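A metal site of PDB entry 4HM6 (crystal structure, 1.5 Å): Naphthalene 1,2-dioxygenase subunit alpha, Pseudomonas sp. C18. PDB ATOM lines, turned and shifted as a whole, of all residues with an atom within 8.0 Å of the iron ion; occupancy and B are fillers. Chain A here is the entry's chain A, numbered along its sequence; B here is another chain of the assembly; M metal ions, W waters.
The backbone carbonyl oxygen (O) of Trp 358 lies close to a ring nitrogen (ND1) of His 213, at 3.3 Å.
A ring nitrogen (ND1) of His 213 is in hydrogen-bond range of the side-chain carboxylate (OD2) of Asp 361, 2.9 Å away.
The side-chain amide oxygen (OD1) of Asn 201 sits close to a ring nitrogen (NE2) of His 208, 3.4 Å away.
ND1 of His 208 sits at hydrogen-bond distance from O of Asp 205.
OD2 of Asp 205 lies close to OD1 of Asn 201, at 3.4 Å.
OD1 of Asn 201 sits at hydrogen-bond distance from OH of Tyr 103 of chain B.
Merely in contact with the iron ion: Asn 201.
Four residues have an atom within 4 Å of the iron ion: Asn 201, His 208, His 213 and Asp 362.
The nearest printed residue that does not touch the iron ion is Thr 212 (4.4 Å).
The iron ion is bound by water W1 (1.9 Å), NE2 of His 213 (2.0 Å), NE2 of His 208 (2.1 Å), OD1 of Asp 362 (2.2 Å) and OD2 of Asp 362 (2.4 Å).
The iron ion has five donor atoms within binding distance.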
ATOM      1  N   ASN A 201     -20.748 -18.553  25.309  1.00  0.00           N
ATOM      2  CA  ASN A 201     -20.123 -17.942  24.145  1.00  0.00           C
ATOM      3  C   ASN A 201     -18.643 -17.676  24.418  1.00  0.00           C
ATOM      4  O   ASN A 201     -17.777 -18.041  23.614  1.00  0.00           O
ATOM      5  CB  ASN A 201     -20.877 -16.660  23.775  1.00  0.00           C
ATOM      6  CG  ASN A 201     -20.304 -15.975  22.552  1.00  0.00           C
ATOM      7  OD1 ASN A 201     -20.689 -16.256  21.418  1.00  0.00           O
ATOM      8  ND2 ASN A 201     -19.383 -15.044  22.782  1.00  0.00           N
ATOM      9  N   PHE A 202     -18.343 -17.066  25.560  1.00  0.00           N
ATOM     10  CA  PHE A 202     -16.947 -16.806  25.910  1.00  0.00           C
ATOM     11  C   PHE A 202     -16.160 -18.063  26.250  1.00  0.00           C
ATOM     12  O   PHE A 202     -14.946 -18.087  26.026  1.00  0.00           O
ATOM     13  CB  PHE A 202     -16.857 -15.812  27.080  1.00  0.00           C
ATOM     14  CG  PHE A 202     -16.941 -14.376  26.655  1.00  0.00           C
ATOM     15  CD1 PHE A 202     -18.114 -13.872  26.102  1.00  0.00           C
ATOM     16  CD2 PHE A 202     -15.861 -13.521  26.805  1.00  0.00           C
ATOM     17  CE1 PHE A 202     -18.209 -12.549  25.691  1.00  0.00           C
ATOM     18  CE2 PHE A 202     -15.944 -12.183  26.410  1.00  0.00           C
ATOM     19  CZ  PHE A 202     -17.122 -11.702  25.851  1.00  0.00           C
ATOM     20  N   ASP A 205     -16.767 -20.493  22.162  1.00  0.00           N
ATOM     21  CA  ASP A 205     -17.350 -20.211  20.861  1.00  0.00           C
ATOM     22  C   ASP A 205     -16.431 -19.404  19.958  1.00  0.00           C
ATOM     23  O   ASP A 205     -16.547 -18.177  19.857  1.00  0.00           O
ATOM     24  CB  ASP A 205     -18.680 -19.490  21.037  1.00  0.00           C
ATOM     25  CG  ASP A 205     -19.544 -19.505  19.788  1.00  0.00           C
ATOM     26  OD1 ASP A 205     -19.008 -19.703  18.678  1.00  0.00           O
ATOM     27  OD2 ASP A 205     -20.758 -19.295  19.932  1.00  0.00           O
ATOM     28  N   HIS A 208     -18.445 -18.678  16.058  1.00  0.00           N
ATOM     29  CA  HIS A 208     -19.305 -17.527  15.748  1.00  0.00           C
ATOM     30  C   HIS A 208     -18.545 -16.316  15.234  1.00  0.00           C
ATOM     31  O   HIS A 208     -19.130 -15.437  14.613  1.00  0.00           O
ATOM     32  CB  HIS A 208     -20.174 -17.128  16.946  1.00  0.00           C
ATOM     33  CG  HIS A 208     -19.505 -16.175  17.897  1.00  0.00           C
ATOM     34  ND1 HIS A 208     -18.437 -16.543  18.697  1.00  0.00           N
ATOM     35  CD2 HIS A 208     -19.762 -14.883  18.199  1.00  0.00           C
ATOM     36  CE1 HIS A 208     -18.068 -15.502  19.429  1.00  0.00           C
ATOM     37  NE2 HIS A 208     -18.854 -14.486  19.146  1.00  0.00           N
ATOM     38  N   VAL A 209     -17.229 -16.256  15.491  1.00  0.00           N
ATOM     39  CA  VAL A 209     -16.488 -15.005  15.324  1.00  0.00           C
ATOM     40  C   VAL A 209     -16.525 -14.426  13.907  1.00  0.00           C
ATOM     41  O   VAL A 209     -16.877 -13.253  13.725  1.00  0.00           O
ATOM     42  CB  VAL A 209     -15.027 -15.120  15.834  1.00  0.00           C
ATOM     43  CG1 VAL A 209     -14.266 -13.820  15.584  1.00  0.00           C
ATOM     44  CG2 VAL A 209     -15.028 -15.467  17.313  1.00  0.00           C
ATOM     45  N   THR A 212     -20.717 -13.713  13.125  1.00  0.00           N
ATOM     46  CA  THR A 212     -21.306 -12.726  14.042  1.00  0.00           C
ATOM     47  C   THR A 212     -20.575 -11.384  13.956  1.00  0.00           C
ATOM     48  O   THR A 212     -21.200 -10.314  13.849  1.00  0.00           O
ATOM     49  CB  THR A 212     -21.289 -13.216  15.504  1.00  0.00           C
ATOM     50  OG1 THR A 212     -22.253 -14.266  15.680  1.00  0.00           O
ATOM     51  CG2 THR A 212     -21.637 -12.073  16.461  1.00  0.00           C
ATOM     52  N   HIS A 213     -19.248 -11.437  14.002  1.00  0.00           N
ATOM     53  CA  HIS A 213     -18.454 -10.226  14.104  1.00  0.00           C
ATOM     54  C   HIS A 213     -17.879  -9.788  12.770  1.00  0.00           C
ATOM     55  O   HIS A 213     -16.910  -9.022  12.735  1.00  0.00           O
ATOM     56  CB  HIS A 213     -17.346 -10.390  15.148  1.00  0.00           C
ATOM     57  CG  HIS A 213     -17.854 -10.608  16.539  1.00  0.00           C
ATOM     58  ND1 HIS A 213     -18.475  -9.608  17.264  1.00  0.00           N
ATOM     59  CD2 HIS A 213     -17.829 -11.702  17.331  1.00  0.00           C
ATOM     60  CE1 HIS A 213     -18.816 -10.090  18.448  1.00  0.00           C
ATOM     61  NE2 HIS A 213     -18.440 -11.348  18.514  1.00  0.00           N
ATOM     62  N   LEU A 307     -11.275 -12.193  27.956  1.00  0.00           N
ATOM     63  CA  LEU A 307     -10.418 -12.399  26.792  1.00  0.00           C
ATOM     64  C   LEU A 307      -9.057 -11.889  27.196  1.00  0.00           C
ATOM     65  O   LEU A 307      -8.879 -10.683  27.341  1.00  0.00           O
ATOM     66  CB  LEU A 307     -10.911 -11.582  25.597  1.00  0.00           C
ATOM     67  CG  LEU A 307     -12.379 -11.784  25.167  1.00  0.00           C
ATOM     68  CD1 LEU A 307     -12.768 -10.898  23.975  1.00  0.00           C
ATOM     69  CD2 LEU A 307     -12.639 -13.238  24.840  1.00  0.00           C
ATOM     70  N   PHE A 352     -15.753  -3.880  23.593  1.00  0.00           N
ATOM     71  CA  PHE A 352     -16.623  -4.757  24.378  1.00  0.00           C
ATOM     72  C   PHE A 352     -17.377  -4.122  25.534  1.00  0.00           C
ATOM     73  O   PHE A 352     -18.026  -4.824  26.316  1.00  0.00           O
ATOM     74  CB  PHE A 352     -15.827  -5.986  24.866  1.00  0.00           C
ATOM     75  CG  PHE A 352     -15.685  -7.055  23.835  1.00  0.00           C
ATOM     76  CD1 PHE A 352     -14.630  -7.034  22.936  1.00  0.00           C
ATOM     77  CD2 PHE A 352     -16.629  -8.061  23.730  1.00  0.00           C
ATOM     78  CE1 PHE A 352     -14.506  -8.009  21.963  1.00  0.00           C
ATOM     79  CE2 PHE A 352     -16.510  -9.054  22.765  1.00  0.00           C
ATOM     80  CZ  PHE A 352     -15.452  -9.028  21.878  1.00  0.00           C
ATOM     81  N   TRP A 358     -18.023  -4.538  18.985  1.00  0.00           N
ATOM     82  CA  TRP A 358     -17.992  -6.003  18.925  1.00  0.00           C
ATOM     83  C   TRP A 358     -19.100  -6.598  19.773  1.00  0.00           C
ATOM     84  O   TRP A 358     -19.868  -7.425  19.310  1.00  0.00           O
ATOM     85  CB  TRP A 358     -16.658  -6.551  19.424  1.00  0.00           C
ATOM     86  CG  TRP A 358     -15.463  -6.299  18.535  1.00  0.00           C
ATOM     87  CD1 TRP A 358     -14.879  -5.100  18.252  1.00  0.00           C
ATOM     88  CD2 TRP A 358     -14.663  -7.297  17.874  1.00  0.00           C
ATOM     89  NE1 TRP A 358     -13.784  -5.284  17.434  1.00  0.00           N
ATOM     90  CE2 TRP A 358     -13.630  -6.629  17.192  1.00  0.00           C
ATOM     91  CE3 TRP A 358     -14.734  -8.688  17.784  1.00  0.00           C
ATOM     92  CZ2 TRP A 358     -12.668  -7.293  16.429  1.00  0.00           C
ATOM     93  CZ3 TRP A 358     -13.774  -9.362  17.025  1.00  0.00           C
ATOM     94  CH2 TRP A 358     -12.760  -8.659  16.363  1.00  0.00           C
ATOM     95  N   GLU A 359     -19.187  -6.160  21.034  1.00  0.00           N
ATOM     96  CA  GLU A 359     -20.197  -6.693  21.943  1.00  0.00           C
ATOM     97  C   GLU A 359     -21.603  -6.543  21.357  1.00  0.00           C
ATOM     98  O   GLU A 359     -22.453  -7.408  21.551  1.00  0.00           O
ATOM     99  CB  GLU A 359     -20.088  -6.001  23.320  1.00  0.00           C
ATOM    100  CG  GLU A 359     -21.139  -6.432  24.349  1.00  0.00           C
ATOM    101  CD  GLU A 359     -20.617  -7.421  25.384  1.00  0.00           C
ATOM    102  OE1 GLU A 359     -19.635  -8.141  25.100  1.00  0.00           O
ATOM    103  OE2 GLU A 359     -21.199  -7.467  26.497  1.00  0.00           O
ATOM    104  N   SER A 360     -21.836  -5.451  20.621  1.00  0.00           N
ATOM    105  CA  SER A 360     -23.155  -5.201  20.052  1.00  0.00           C
ATOM    106  C   SER A 360     -23.539  -6.248  19.010  1.00  0.00           C
ATOM    107  O   SER A 360     -24.738  -6.563  18.858  1.00  0.00           O
ATOM    108  CB  SER A 360     -23.248  -3.789  19.460  1.00  0.00           C
ATOM    109  OG  SER A 360     -22.544  -3.684  18.229  1.00  0.00           O
ATOM    110  N   ASP A 361     -22.554  -6.800  18.314  1.00  0.00           N
ATOM    111  CA  ASP A 361     -22.812  -7.851  17.323  1.00  0.00           C
ATOM    112  C   ASP A 361     -23.455  -9.068  17.983  1.00  0.00           C
ATOM    113  O   ASP A 361     -24.165  -9.837  17.319  1.00  0.00           O
ATOM    114  CB  ASP A 361     -21.519  -8.329  16.658  1.00  0.00           C
ATOM    115  CG  ASP A 361     -20.746  -7.222  15.930  1.00  0.00           C
ATOM    116  OD1 ASP A 361     -21.355  -6.238  15.470  1.00  0.00           O
ATOM    117  OD2 ASP A 361     -19.518  -7.381  15.810  1.00  0.00           O
ATOM    118  N   ASP A 362     -23.174  -9.266  19.267  1.00  0.00           N
ATOM    119  CA  ASP A 362     -23.630 -10.472  19.962  1.00  0.00           C
ATOM    120  C   ASP A 362     -25.034 -10.336  20.548  1.00  0.00           C
ATOM    121  O   ASP A 362     -25.636 -11.342  20.888  1.00  0.00           O
ATOM    122  CB  ASP A 362     -22.679 -10.819  21.125  1.00  0.00           C
ATOM    123  CG  ASP A 362     -21.343 -11.363  20.663  1.00  0.00           C
ATOM    124  OD1 ASP A 362     -21.316 -12.458  20.067  1.00  0.00           O
ATOM    125  OD2 ASP A 362     -20.321 -10.704  20.923  1.00  0.00           O
ATOM    126  N   ASN A 363     -25.533  -9.102  20.679  1.00  0.00           N
ATOM    127  CA  ASN A 363     -26.784  -8.838  21.405  1.00  0.00           C
ATOM    128  C   ASN A 363     -27.957  -9.694  20.947  1.00  0.00           C
ATOM    129  O   ASN A 363     -28.560 -10.389  21.765  1.00  0.00           O
ATOM    130  CB  ASN A 363     -27.223  -7.381  21.256  1.00  0.00           C
ATOM    131  CG  ASN A 363     -26.493  -6.440  22.180  1.00  0.00           C
ATOM    132  OD1 ASN A 363     -26.697  -5.227  22.112  1.00  0.00           O
ATOM    133  ND2 ASN A 363     -25.632  -6.972  23.045  1.00  0.00           N
ATOM    134  N   ASN A 365     -28.066 -12.308  19.064  1.00  0.00           N
ATOM    135  CA  ASN A 365     -27.777 -13.725  19.236  1.00  0.00           C
ATOM    136  C   ASN A 365     -28.102 -14.203  20.647  1.00  0.00           C
ATOM    137  O   ASN A 365     -28.832 -15.178  20.818  1.00  0.00           O
ATOM    138  CB  ASN A 365     -26.308 -14.040  18.910  1.00  0.00           C
ATOM    139  CG  ASN A 365     -25.960 -13.800  17.443  1.00  0.00           C
ATOM    140  OD1 ASN A 365     -26.819 -13.871  16.560  1.00  0.00           O
ATOM    141  ND2 ASN A 365     -24.686 -13.544  17.177  1.00  0.00           N
ATOM    142  N   MET A 366     -27.590 -13.521  21.666  1.00  0.00           N
ATOM    143  CA  MET A 366     -27.836 -13.987  23.037  1.00  0.00           C
ATOM    144  C   MET A 366     -29.259 -13.766  23.500  1.00  0.00           C
ATOM    145  O   MET A 366     -29.814 -14.613  24.216  1.00  0.00           O
ATOM    146  CB  MET A 366     -26.940 -13.309  24.068  1.00  0.00           C
ATOM    147  CG  MET A 366     -25.810 -12.546  23.526  1.00  0.00           C
ATOM    148  SD  MET A 366     -24.337 -13.165  24.285  1.00  0.00           S
ATOM    149  CE  MET A 366     -24.553 -14.874  23.844  1.00  0.00           C
ATOM    150  N   TYR B 103     -25.733 -16.124  13.837  1.00  0.00           N
ATOM    151  CA  TYR B 103     -24.870 -16.523  14.942  1.00  0.00           C
ATOM    152  C   TYR B 103     -23.655 -17.289  14.394  1.00  0.00           C
ATOM    153  O   TYR B 103     -22.528 -16.762  14.390  1.00  0.00           O
ATOM    154  CB  TYR B 103     -25.659 -17.308  15.984  1.00  0.00           C
ATOM    155  CG  TYR B 103     -25.042 -17.368  17.385  1.00  0.00           C
ATOM    156  CD1 TYR B 103     -23.717 -17.002  17.613  1.00  0.00           C
ATOM    157  CD2 TYR B 103     -25.791 -17.792  18.464  1.00  0.00           C
ATOM    158  CE1 TYR B 103     -23.160 -17.063  18.878  1.00  0.00           C
ATOM    159  CE2 TYR B 103     -25.249 -17.859  19.734  1.00  0.00           C
ATOM    160  CZ  TYR B 103     -23.933 -17.490  19.939  1.00  0.00           C
ATOM    161  OH  TYR B 103     -23.385 -17.562  21.201  1.00  0.00           O
HETATM  162 FE    FE M   1     -19.094 -12.569  19.998  1.00  0.00          FE
HETATM  163  O   HOH W   1     -18.499 -12.916  21.806  1.00  0.00           O
